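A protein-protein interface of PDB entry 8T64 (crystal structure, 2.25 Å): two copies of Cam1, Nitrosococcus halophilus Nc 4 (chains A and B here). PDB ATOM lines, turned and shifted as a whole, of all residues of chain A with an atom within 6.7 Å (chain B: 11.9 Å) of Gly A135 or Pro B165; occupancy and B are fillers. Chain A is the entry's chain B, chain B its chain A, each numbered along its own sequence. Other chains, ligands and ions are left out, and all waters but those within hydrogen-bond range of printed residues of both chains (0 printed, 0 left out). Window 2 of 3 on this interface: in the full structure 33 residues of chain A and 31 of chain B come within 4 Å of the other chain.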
ATOM      1  N   ILE A 112      11.843 -29.719 -29.602  1.00  0.00           N
ATOM      2  CA  ILE A 112      11.127 -28.467 -29.376  1.00  0.00           C
ATOM      3  C   ILE A 112      10.714 -28.378 -27.912  1.00  0.00           C
ATOM      4  O   ILE A 112      10.307 -29.378 -27.308  1.00  0.00           O
ATOM      5  CB  ILE A 112       9.881 -28.348 -30.281  1.00  0.00           C
ATOM      6  CG1 ILE A 112      10.214 -28.720 -31.712  1.00  0.00           C
ATOM      7  CG2 ILE A 112       9.307 -26.929 -30.233  1.00  0.00           C
ATOM      8  CD1 ILE A 112       9.056 -28.543 -32.642  1.00  0.00           C
ATOM      9  N   ALA A 130      -1.183 -26.793 -25.089  1.00  0.00           N
ATOM     10  CA  ALA A 130      -0.692 -27.188 -26.413  1.00  0.00           C
ATOM     11  C   ALA A 130       0.523 -28.099 -26.301  1.00  0.00           C
ATOM     12  O   ALA A 130       0.643 -29.080 -27.045  1.00  0.00           O
ATOM     13  CB  ALA A 130      -0.349 -25.954 -27.254  1.00  0.00           C
ATOM     14  N   ALA A 131       1.412 -27.809 -25.351  1.00  0.00           N
ATOM     15  CA  ALA A 131       2.650 -28.557 -25.177  1.00  0.00           C
ATOM     16  C   ALA A 131       2.422 -29.932 -24.557  1.00  0.00           C
ATOM     17  O   ALA A 131       3.139 -30.885 -24.892  1.00  0.00           O
ATOM     18  CB  ALA A 131       3.624 -27.762 -24.314  1.00  0.00           C
ATOM     19  N   GLU A 132       1.463 -30.045 -23.634  1.00  0.00           N
ATOM     20  CA  GLU A 132       1.100 -31.360 -23.117  1.00  0.00           C
ATOM     21  C   GLU A 132       0.443 -32.199 -24.200  1.00  0.00           C
ATOM     22  O   GLU A 132       0.686 -33.405 -24.297  1.00  0.00           O
ATOM     23  CB  GLU A 132       0.159 -31.215 -21.916  1.00  0.00           C
ATOM     24  CG  GLU A 132       0.896 -30.863 -20.636  1.00  0.00           C
ATOM     25  CD  GLU A 132       1.740 -32.004 -20.170  1.00  0.00           C
ATOM     26  OE1 GLU A 132       1.240 -33.153 -20.231  1.00  0.00           O
ATOM     27  OE2 GLU A 132       2.899 -31.768 -19.778  1.00  0.00           O
ATOM     28  N   GLU A 133      -0.378 -31.564 -25.028  1.00  0.00           N
ATOM     29  CA  GLU A 133      -1.151 -32.249 -26.043  1.00  0.00           C
ATOM     30  C   GLU A 133      -0.295 -32.694 -27.214  1.00  0.00           C
ATOM     31  O   GLU A 133      -0.691 -33.619 -27.925  1.00  0.00           O
ATOM     32  CB  GLU A 133      -2.294 -31.333 -26.496  1.00  0.00           C
ATOM     33  CG  GLU A 133      -3.026 -31.729 -27.774  1.00  0.00           C
ATOM     34  CD  GLU A 133      -3.448 -30.517 -28.589  1.00  0.00           C
ATOM     35  OE1 GLU A 133      -2.626 -30.019 -29.397  1.00  0.00           O
ATOM     36  OE2 GLU A 133      -4.592 -30.039 -28.394  1.00  0.00           O
ATOM     37  N   ALA A 134       0.877 -32.091 -27.411  1.00  0.00           N
ATOM     38  CA  ALA A 134       1.805 -32.517 -28.452  1.00  0.00           C
ATOM     39  C   ALA A 134       2.978 -33.294 -27.897  1.00  0.00           C
ATOM     40  O   ALA A 134       3.845 -33.715 -28.670  1.00  0.00           O
ATOM     41  CB  ALA A 134       2.322 -31.316 -29.252  1.00  0.00           C
ATOM     42  N   GLY A 135       3.034 -33.482 -26.583  1.00  0.00           N
ATOM     43  CA  GLY A 135       4.114 -34.242 -25.990  1.00  0.00           C
ATOM     44  C   GLY A 135       5.454 -33.547 -25.909  1.00  0.00           C
ATOM     45  O   GLY A 135       6.479 -34.230 -25.897  1.00  0.00           O
ATOM     46  N   VAL A 136       5.492 -32.216 -25.815  1.00  0.00           N
ATOM     47  CA  VAL A 136       6.766 -31.503 -25.727  1.00  0.00           C
ATOM     48  C   VAL A 136       6.950 -30.933 -24.324  1.00  0.00           C
ATOM     49  O   VAL A 136       6.016 -30.833 -23.527  1.00  0.00           O
ATOM     50  CB  VAL A 136       6.917 -30.397 -26.797  1.00  0.00           C
ATOM     51  CG1 VAL A 136       6.684 -30.971 -28.217  1.00  0.00           C
ATOM     52  CG2 VAL A 136       5.985 -29.251 -26.521  1.00  0.00           C
ATOM     53  N   ALA A 137       8.192 -30.574 -24.021  1.00  0.00           N
ATOM     54  CA  ALA A 137       8.552 -30.109 -22.692  1.00  0.00           C
ATOM     55  C   ALA A 137       8.196 -28.640 -22.519  1.00  0.00           C
ATOM     56  O   ALA A 137       8.386 -27.826 -23.427  1.00  0.00           O
ATOM     57  CB  ALA A 137      10.043 -30.308 -22.438  1.00  0.00           C
ATOM     58  N   SER A 138       7.672 -28.313 -21.344  1.00  0.00           N
ATOM     59  CA  SER A 138       7.388 -26.938 -20.954  1.00  0.00           C
ATOM     60  C   SER A 138       8.515 -26.411 -20.076  1.00  0.00           C
ATOM     61  O   SER A 138       9.013 -27.124 -19.199  1.00  0.00           O
ATOM     62  CB  SER A 138       6.060 -26.853 -20.198  1.00  0.00           C
ATOM     63  OG  SER A 138       4.985 -27.248 -21.021  1.00  0.00           O
ATOM     64  N   PRO B  90       6.307 -26.717  -9.585  1.00  0.00           N
ATOM     65  CA  PRO B  90       4.859 -26.941  -9.727  1.00  0.00           C
ATOM     66  C   PRO B  90       4.374 -28.232  -9.093  1.00  0.00           C
ATOM     67  O   PRO B  90       3.169 -28.353  -8.828  1.00  0.00           O
ATOM     68  CB  PRO B  90       4.637 -26.934 -11.245  1.00  0.00           C
ATOM     69  CG  PRO B  90       5.980 -27.156 -11.844  1.00  0.00           C
ATOM     70  CD  PRO B  90       6.997 -26.648 -10.888  1.00  0.00           C
ATOM     71  N   ARG B  94       0.859 -28.569  -7.068  1.00  0.00           N
ATOM     72  CA  ARG B  94      -0.042 -29.644  -7.470  1.00  0.00           C
ATOM     73  C   ARG B  94      -0.438 -30.499  -6.276  1.00  0.00           C
ATOM     74  O   ARG B  94      -1.616 -30.800  -6.086  1.00  0.00           O
ATOM     75  CB  ARG B  94       0.615 -30.509  -8.561  1.00  0.00           C
ATOM     76  CG  ARG B  94      -0.342 -31.550  -9.213  1.00  0.00           C
ATOM     77  CD  ARG B  94       0.370 -32.613 -10.083  1.00  0.00           C
ATOM     78  NE  ARG B  94       1.291 -33.449  -9.310  1.00  0.00           N
ATOM     79  CZ  ARG B  94       2.540 -33.773  -9.669  1.00  0.00           C
ATOM     80  NH1 ARG B  94       3.274 -34.538  -8.865  1.00  0.00           N
ATOM     81  NH2 ARG B  94       3.074 -33.340 -10.814  1.00  0.00           N
ATOM     82  N   LEU B 125       0.205 -23.246 -12.348  1.00  0.00           N
ATOM     83  CA  LEU B 125       0.273 -24.419 -13.219  1.00  0.00           C
ATOM     84  C   LEU B 125       0.187 -25.701 -12.420  1.00  0.00           C
ATOM     85  O   LEU B 125      -0.435 -26.666 -12.861  1.00  0.00           O
ATOM     86  CB  LEU B 125       1.578 -24.429 -14.027  1.00  0.00           C
ATOM     87  CG  LEU B 125       1.809 -23.415 -15.141  1.00  0.00           C
ATOM     88  CD1 LEU B 125       3.134 -23.671 -15.823  1.00  0.00           C
ATOM     89  CD2 LEU B 125       0.728 -23.558 -16.142  1.00  0.00           C
ATOM     90  N   MET B 129      -2.630 -28.447 -12.958  1.00  0.00           N
ATOM     91  CA  MET B 129      -2.405 -29.885 -13.023  1.00  0.00           C
ATOM     92  C   MET B 129      -3.260 -30.622 -11.997  1.00  0.00           C
ATOM     93  O   MET B 129      -3.913 -31.623 -12.325  1.00  0.00           O
ATOM     94  CB  MET B 129      -0.914 -30.192 -12.829  1.00  0.00           C
ATOM     95  CG  MET B 129      -0.054 -29.887 -14.076  1.00  0.00           C
ATOM     96  SD  MET B 129       1.705 -30.143 -13.764  1.00  0.00           S
ATOM     97  CE  MET B 129       2.454 -28.844 -14.734  1.00  0.00           C
ATOM     98  N   ARG B 160      13.836 -23.922 -15.657  1.00  0.00           N
ATOM     99  CA  ARG B 160      13.337 -25.189 -15.150  1.00  0.00           C
ATOM    100  C   ARG B 160      12.410 -25.841 -16.161  1.00  0.00           C
ATOM    101  O   ARG B 160      11.685 -25.160 -16.891  1.00  0.00           O
ATOM    102  CB  ARG B 160      12.594 -24.989 -13.834  1.00  0.00           C
ATOM    103  CG  ARG B 160      13.200 -23.912 -12.983  1.00  0.00           C
ATOM    104  CD  ARG B 160      13.647 -24.479 -11.651  1.00  0.00           C
ATOM    105  NE  ARG B 160      14.315 -23.472 -10.837  1.00  0.00           N
ATOM    106  CZ  ARG B 160      14.224 -23.407  -9.514  1.00  0.00           C
ATOM    107  NH1 ARG B 160      14.867 -22.445  -8.862  1.00  0.00           N
ATOM    108  NH2 ARG B 160      13.484 -24.294  -8.852  1.00  0.00           N
ATOM    109  N   GLN B 161      12.403 -27.165 -16.164  1.00  0.00           N
ATOM    110  CA  GLN B 161      11.526 -27.960 -17.006  1.00  0.00           C
ATOM    111  C   GLN B 161      10.356 -28.270 -16.109  1.00  0.00           C
ATOM    112  O   GLN B 161      10.523 -28.778 -15.038  1.00  0.00           O
ATOM    113  CB  GLN B 161      12.209 -29.226 -17.507  1.00  0.00           C
ATOM    114  CG  GLN B 161      11.692 -29.761 -18.823  1.00  0.00           C
ATOM    115  CD  GLN B 161      12.621 -30.749 -19.493  1.00  0.00           C
ATOM    116  OE1 GLN B 161      13.709 -30.412 -19.899  1.00  0.00           O
ATOM    117  NE2 GLN B 161      12.177 -31.968 -19.628  1.00  0.00           N
ATOM    118  N   ILE B 162       9.163 -27.959 -16.571  1.00  0.00           N
ATOM    119  CA  ILE B 162       7.965 -28.089 -15.793  1.00  0.00           C
ATOM    120  C   ILE B 162       7.081 -29.272 -16.117  1.00  0.00           C
ATOM    121  O   ILE B 162       6.216 -29.609 -15.367  1.00  0.00           O
ATOM    122  CB  ILE B 162       7.182 -26.795 -15.944  1.00  0.00           C
ATOM    123  CG1 ILE B 162       7.557 -25.860 -14.827  1.00  0.00           C
ATOM    124  CG2 ILE B 162       5.700 -27.027 -15.967  1.00  0.00           C
ATOM    125  CD1 ILE B 162       6.893 -24.523 -14.946  1.00  0.00           C
ATOM    126  N   SER B 163       7.299 -29.877 -17.259  1.00  0.00           N
ATOM    127  CA  SER B 163       6.568 -31.035 -17.704  1.00  0.00           C
ATOM    128  C   SER B 163       7.513 -31.643 -18.682  1.00  0.00           C
ATOM    129  O   SER B 163       7.981 -30.990 -19.562  1.00  0.00           O
ATOM    130  CB  SER B 163       5.251 -30.691 -18.394  1.00  0.00           C
ATOM    131  OG  SER B 163       5.350 -30.674 -19.819  1.00  0.00           O
ATOM    132  N   GLN B 164       7.772 -32.914 -18.519  1.00  0.00           N
ATOM    133  CA  GLN B 164       8.696 -33.632 -19.360  1.00  0.00           C
ATOM    134  C   GLN B 164       7.969 -34.865 -19.811  1.00  0.00           C
ATOM    135  O   GLN B 164       8.195 -35.936 -19.278  1.00  0.00           O
ATOM    136  CB  GLN B 164       9.907 -34.005 -18.508  1.00  0.00           C
ATOM    137  CG  GLN B 164      10.767 -35.180 -18.961  1.00  0.00           C
ATOM    138  CD  GLN B 164      12.139 -35.141 -18.320  1.00  0.00           C
ATOM    139  OE1 GLN B 164      12.769 -34.100 -18.261  1.00  0.00           O
ATOM    140  NE2 GLN B 164      12.593 -36.269 -17.823  1.00  0.00           N
ATOM    141  N   PRO B 165       7.064 -34.712 -20.772  1.00  0.00           N
ATOM    142  CA  PRO B 165       6.279 -35.824 -21.281  1.00  0.00           C
ATOM    143  C   PRO B 165       6.911 -36.417 -22.534  1.00  0.00           C
ATOM    144  O   PRO B 165       7.592 -35.683 -23.237  1.00  0.00           O
ATOM    145  CB  PRO B 165       4.945 -35.154 -21.628  1.00  0.00           C
ATOM    146  CG  PRO B 165       5.169 -33.679 -21.517  1.00  0.00           C
ATOM    147  CD  PRO B 165       6.634 -33.468 -21.403  1.00  0.00           C
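Printed residues of chain B within 4 Å of Gly A135: Pro B165 (3.2 Å). No residue of chain B comes within 4 Å of Ala A131. No residue of chain B comes within 4 Å of Ala A134. Val A136 touches two residues of chain B. Of chain B, only Gln B161, Ile B162 and Ser B163 come within 4 Å of Ser A138. Of the printed residues of chain A, Gln B161 touches Ala A137 (3.9 Å) and Ser A138 (3.4 Å). Of the printed residues of chain A, Ile B162 touches Ser A138. Printed residues of chain A within 4 Å of Ser B163: Glu A132 (2.7 Å), Val A136 (3.8 Å), Ala A137 (3.3 Å) and Ser A138 (3.2 Å). The nearest residue of chain B that does not touch Gly A135 is Gln B164 (6.3 Å). The nearest residue of chain A that does not touch Pro B165 is Ala A137 (4.1 Å). The nearest printed residue of chain A that does not touch Ile B162 is Glu A132 (5.9 Å).
Among the printed residues, merely in contact across the chains: Glu A132 with Pro B165 (3.4 Å), Val A136 with Ser B163 (3.8 Å), Val A136 with Pro B165 (3.4 Å), Ala A137 with Gln B161 (3.9 Å), Ala A137 with Ser B163 (3.3 Å) and Ser A138 with Gln B161 (3.4 Å).
Printed residues of chain B that touch a printed residue of chain A: Gln B161, Ile B162, Ser B163 and Pro B165. Hydrophobic or aromatic side chains of chain B that line the printed part of chain A: Ile B162 and Pro B165. Among the printed residues, 10 pairs touch across the chains. Among the printed residues, no Asp or Glu carboxylate lies within 4 Å of a Lys or Arg side-chain nitrogen of the other chain.
No position is printed for both chains. Of the 10 pairs that touch across the chains among the printed residues, none has its exchanged pair printed and touching as well.
The side-chain amide oxygen of Gln B164 sits at hydrogen-bond distance from the side-chain amide nitrogen of Gln B161 (2.6 Å). O of Ala A131 is in hydrogen-bond range of N of Val A136, at 2.9 Å.
The side-chain carboxylate (OE2) of Glu A132 is in hydrogen-bond range of the side-chain hydroxyl (OG) of Ser B163, at 2.7 Å. The backbone NH (N) of Ile B162 sits at hydrogen-bond distance from the backbone carbonyl oxygen (O) of Ser A138 (2.8 Å). O of Ser B163 is in hydrogen-bond range of N of Ser A138, 3.2 Å away. The backbone carbonyl oxygen of Pro B165 sits close to the backbone carbonyl oxygen of Gly A135 (3.2 Å).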
